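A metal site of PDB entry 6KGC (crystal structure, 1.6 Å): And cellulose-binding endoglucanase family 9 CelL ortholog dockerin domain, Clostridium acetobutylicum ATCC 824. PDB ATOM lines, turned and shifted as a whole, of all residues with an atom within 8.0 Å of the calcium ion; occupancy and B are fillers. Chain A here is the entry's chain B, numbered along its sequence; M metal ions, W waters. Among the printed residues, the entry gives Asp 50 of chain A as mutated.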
ATOM      1  N   MET A  22     -15.979 -23.734 -12.926  1.00  0.00           N
ATOM      2  CA  MET A  22     -14.733 -23.009 -12.688  1.00  0.00           C
ATOM      3  C   MET A  22     -14.655 -22.508 -11.249  1.00  0.00           C
ATOM      4  O   MET A  22     -13.604 -22.616 -10.589  1.00  0.00           O
ATOM      5  CB  MET A  22     -14.603 -21.844 -13.665  1.00  0.00           C
ATOM      6  CG  MET A  22     -13.368 -21.008 -13.478  1.00  0.00           C
ATOM      7  SD  MET A  22     -11.828 -21.849 -13.879  1.00  0.00           S
ATOM      8  CE  MET A  22     -11.836 -21.610 -15.675  1.00  0.00           C
ATOM      9  N   LEU A  39      -9.482 -25.734 -18.754  1.00  0.00           N
ATOM     10  CA  LEU A  39      -9.432 -24.799 -17.638  1.00  0.00           C
ATOM     11  C   LEU A  39      -8.567 -23.582 -17.932  1.00  0.00           C
ATOM     12  O   LEU A  39      -8.937 -22.456 -17.566  1.00  0.00           O
ATOM     13  CB  LEU A  39      -8.932 -25.509 -16.381  1.00  0.00           C
ATOM     14  CG  LEU A  39      -9.928 -26.498 -15.783  1.00  0.00           C
ATOM     15  CD1 LEU A  39      -9.263 -27.369 -14.722  1.00  0.00           C
ATOM     16  CD2 LEU A  39     -11.095 -25.781 -15.165  1.00  0.00           C
ATOM     17  N   ASP A  40      -7.417 -23.771 -18.586  1.00  0.00           N
ATOM     18  CA  ASP A  40      -6.476 -22.675 -18.801  1.00  0.00           C
ATOM     19  C   ASP A  40      -6.839 -21.874 -20.049  1.00  0.00           C
ATOM     20  O   ASP A  40      -6.206 -21.982 -21.110  1.00  0.00           O
ATOM     21  CB  ASP A  40      -5.049 -23.219 -18.886  1.00  0.00           C
ATOM     22  CG  ASP A  40      -4.016 -22.126 -19.015  1.00  0.00           C
ATOM     23  OD1 ASP A  40      -4.359 -20.964 -18.728  1.00  0.00           O
ATOM     24  OD2 ASP A  40      -2.877 -22.450 -19.426  1.00  0.00           O
ATOM     25  N   ILE A  41      -7.840 -21.010 -19.892  1.00  0.00           N
ATOM     26  CA  ILE A  41      -8.448 -20.352 -21.050  1.00  0.00           C
ATOM     27  C   ILE A  41      -7.491 -19.348 -21.690  1.00  0.00           C
ATOM     28  O   ILE A  41      -7.503 -19.167 -22.914  1.00  0.00           O
ATOM     29  CB  ILE A  41      -9.771 -19.695 -20.624  1.00  0.00           C
ATOM     30  CG1 ILE A  41     -10.732 -20.763 -20.126  1.00  0.00           C
ATOM     31  CG2 ILE A  41     -10.361 -18.888 -21.765  1.00  0.00           C
ATOM     32  CD1 ILE A  41     -11.980 -20.195 -19.520  1.00  0.00           C
ATOM     33  N   ASN A  42      -6.681 -18.657 -20.891  1.00  0.00           N
ATOM     34  CA  ASN A  42      -5.764 -17.665 -21.468  1.00  0.00           C
ATOM     35  C   ASN A  42      -4.372 -18.249 -21.757  1.00  0.00           C
ATOM     36  O   ASN A  42      -3.489 -17.502 -22.183  1.00  0.00           O
ATOM     37  CB  ASN A  42      -5.643 -16.432 -20.568  1.00  0.00           C
ATOM     38  CG  ASN A  42      -5.167 -16.741 -19.155  1.00  0.00           C
ATOM     39  OD1 ASN A  42      -4.612 -17.802 -18.887  1.00  0.00           O
ATOM     40  ND2 ASN A  42      -5.372 -15.791 -18.250  1.00  0.00           N
ATOM     41  N   GLY A  43      -4.179 -19.550 -21.558  1.00  0.00           N
ATOM     42  CA  GLY A  43      -2.975 -20.248 -21.951  1.00  0.00           C
ATOM     43  C   GLY A  43      -1.699 -19.833 -21.253  1.00  0.00           C
ATOM     44  O   GLY A  43      -0.623 -20.049 -21.800  1.00  0.00           O
ATOM     45  N   ASP A  44      -1.775 -19.252 -20.055  1.00  0.00           N
ATOM     46  CA  ASP A  44      -0.565 -18.777 -19.388  1.00  0.00           C
ATOM     47  C   ASP A  44       0.041 -19.812 -18.436  1.00  0.00           C
ATOM     48  O   ASP A  44       0.996 -19.490 -17.722  1.00  0.00           O
ATOM     49  CB  ASP A  44      -0.863 -17.452 -18.674  1.00  0.00           C
ATOM     50  CG  ASP A  44      -1.787 -17.601 -17.487  1.00  0.00           C
ATOM     51  OD1 ASP A  44      -2.263 -18.727 -17.233  1.00  0.00           O
ATOM     52  OD2 ASP A  44      -2.016 -16.580 -16.768  1.00  0.00           O
ATOM     53  N   GLY A  45      -0.452 -21.063 -18.458  1.00  0.00           N
ATOM     54  CA  GLY A  45       0.132 -22.149 -17.685  1.00  0.00           C
ATOM     55  C   GLY A  45      -0.505 -22.379 -16.325  1.00  0.00           C
ATOM     56  O   GLY A  45      -0.230 -23.431 -15.706  1.00  0.00           O
ATOM     57  N   ALA A  46      -1.320 -21.456 -15.856  1.00  0.00           N
ATOM     58  CA  ALA A  46      -1.930 -21.529 -14.550  1.00  0.00           C
ATOM     59  C   ALA A  46      -3.445 -21.452 -14.708  1.00  0.00           C
ATOM     60  O   ALA A  46      -3.939 -20.817 -15.638  1.00  0.00           O
ATOM     61  CB  ALA A  46      -1.446 -20.392 -13.655  1.00  0.00           C
ATOM     62  N   VAL A  47      -4.160 -22.083 -13.790  1.00  0.00           N
ATOM     63  CA  VAL A  47      -5.602 -21.909 -13.655  1.00  0.00           C
ATOM     64  C   VAL A  47      -5.859 -20.997 -12.461  1.00  0.00           C
ATOM     65  O   VAL A  47      -5.556 -21.355 -11.327  1.00  0.00           O
ATOM     66  CB  VAL A  47      -6.333 -23.252 -13.506  1.00  0.00           C
ATOM     67  CG1 VAL A  47      -7.850 -23.057 -13.392  1.00  0.00           C
ATOM     68  CG2 VAL A  47      -5.979 -24.139 -14.696  1.00  0.00           C
ATOM     69  N   ASN A  48      -6.433 -19.831 -12.720  1.00  0.00           N
ATOM     70  CA  ASN A  48      -6.679 -18.892 -11.628  1.00  0.00           C
ATOM     71  C   ASN A  48      -7.830 -17.953 -12.002  1.00  0.00           C
ATOM     72  O   ASN A  48      -8.560 -18.184 -12.962  1.00  0.00           O
ATOM     73  CB  ASN A  48      -5.403 -18.109 -11.273  1.00  0.00           C
ATOM     74  CG  ASN A  48      -4.824 -17.300 -12.444  1.00  0.00           C
ATOM     75  OD1 ASN A  48      -5.534 -16.854 -13.336  1.00  0.00           O
ATOM     76  ND2 ASN A  48      -3.494 -17.140 -12.441  1.00  0.00           N
ATOM     77  N   GLY A  49      -8.000 -16.920 -11.186  1.00  0.00           N
ATOM     78  CA  GLY A  49      -9.095 -15.997 -11.388  1.00  0.00           C
ATOM     79  C   GLY A  49      -9.097 -15.294 -12.713  1.00  0.00           C
ATOM     80  O   GLY A  49     -10.145 -14.818 -13.146  1.00  0.00           O
ATOM     81  N   ASP A  50      -7.952 -15.199 -13.385  1.00  0.00           N
ATOM     82  CA  ASP A  50      -7.954 -14.577 -14.716  1.00  0.00           C
ATOM     83  C   ASP A  50      -8.660 -15.460 -15.735  1.00  0.00           C
ATOM     84  O   ASP A  50      -9.299 -14.955 -16.665  1.00  0.00           O
ATOM     85  CB  ASP A  50      -6.534 -14.267 -15.164  1.00  0.00           C
ATOM     86  CG  ASP A  50      -5.869 -13.170 -14.343  1.00  0.00           C
ATOM     87  OD1 ASP A  50      -6.566 -12.264 -13.853  1.00  0.00           O
ATOM     88  OD2 ASP A  50      -4.622 -13.216 -14.184  1.00  0.00           O
ATOM     89  N   ASP A  51      -8.569 -16.777 -15.593  1.00  0.00           N
ATOM     90  CA  ASP A  51      -9.322 -17.670 -16.479  1.00  0.00           C
ATOM     91  C   ASP A  51     -10.812 -17.568 -16.208  1.00  0.00           C
ATOM     92  O   ASP A  51     -11.606 -17.576 -17.157  1.00  0.00           O
ATOM     93  CB  ASP A  51      -8.827 -19.099 -16.308  1.00  0.00           C
ATOM     94  CG  ASP A  51      -7.348 -19.240 -16.601  1.00  0.00           C
ATOM     95  OD1 ASP A  51      -6.953 -19.020 -17.764  1.00  0.00           O
ATOM     96  OD2 ASP A  51      -6.567 -19.554 -15.667  1.00  0.00           O
ATOM     97  N   LEU A  52     -11.214 -17.441 -14.943  1.00  0.00           N
ATOM     98  CA  LEU A  52     -12.613 -17.220 -14.634  1.00  0.00           C
ATOM     99  C   LEU A  52     -13.108 -15.943 -15.282  1.00  0.00           C
ATOM    100  O   LEU A  52     -14.203 -15.897 -15.857  1.00  0.00           O
ATOM    101  CB  LEU A  52     -12.842 -17.176 -13.124  1.00  0.00           C
ATOM    102  CG  LEU A  52     -14.256 -16.818 -12.641  1.00  0.00           C
ATOM    103  CD1 LEU A  52     -15.290 -17.793 -13.150  1.00  0.00           C
ATOM    104  CD2 LEU A  52     -14.284 -16.753 -11.090  1.00  0.00           C
ATOM    105  N   GLU A  54     -11.959 -14.522 -17.977  1.00  0.00           N
ATOM    106  CA  GLU A  54     -12.094 -14.762 -19.404  1.00  0.00           C
ATOM    107  C   GLU A  54     -13.327 -15.611 -19.724  1.00  0.00           C
ATOM    108  O   GLU A  54     -13.941 -15.436 -20.772  1.00  0.00           O
ATOM    109  CB  GLU A  54     -10.851 -15.439 -19.974  1.00  0.00           C
ATOM    110  CG  GLU A  54      -9.564 -14.613 -19.908  1.00  0.00           C
ATOM    111  CD  GLU A  54      -9.519 -13.455 -20.886  1.00  0.00           C
ATOM    112  OE1 GLU A  54     -10.585 -13.028 -21.393  1.00  0.00           O
ATOM    113  OE2 GLU A  54      -8.402 -12.964 -21.154  1.00  0.00           O
HETATM  114 CA    CA M   1      -4.617 -19.254 -17.085  1.00  0.00          CA
HETATM  115  O   HOH W   1      -4.383 -17.312 -15.826  1.00  0.00           O
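The side-chain carboxylate (OD1) of Asp 51 lies close to the backbone NH (N) of Ile 41. OD2 of Asp 40 is in hydrogen-bond range of N of Gly 45 (3.0 Å). N of Asn 48 sits close to OD2 of Asp 51 (3.0 Å). The side-chain carboxylate (OD1) of Asp 40 lies close to the backbone NH (N) of Gly 43 (3.2 Å).
The calcium ion is bound by O of Ala 46, OD1 of Asn 42, water W1, OD1 of Asp 40, OD1 of Asp 44, OD2 of Asp 51 and OD1 of Asp 51. The calcium ion has seven donor atoms within binding distance.
Water W1 lies within hydrogen-bond range of the side-chain carboxylate (OD2) of Asp 44, the side-chain amide oxygen (OD1) of Asn 48 and the side-chain amide nitrogen (ND2) of Asn 42.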
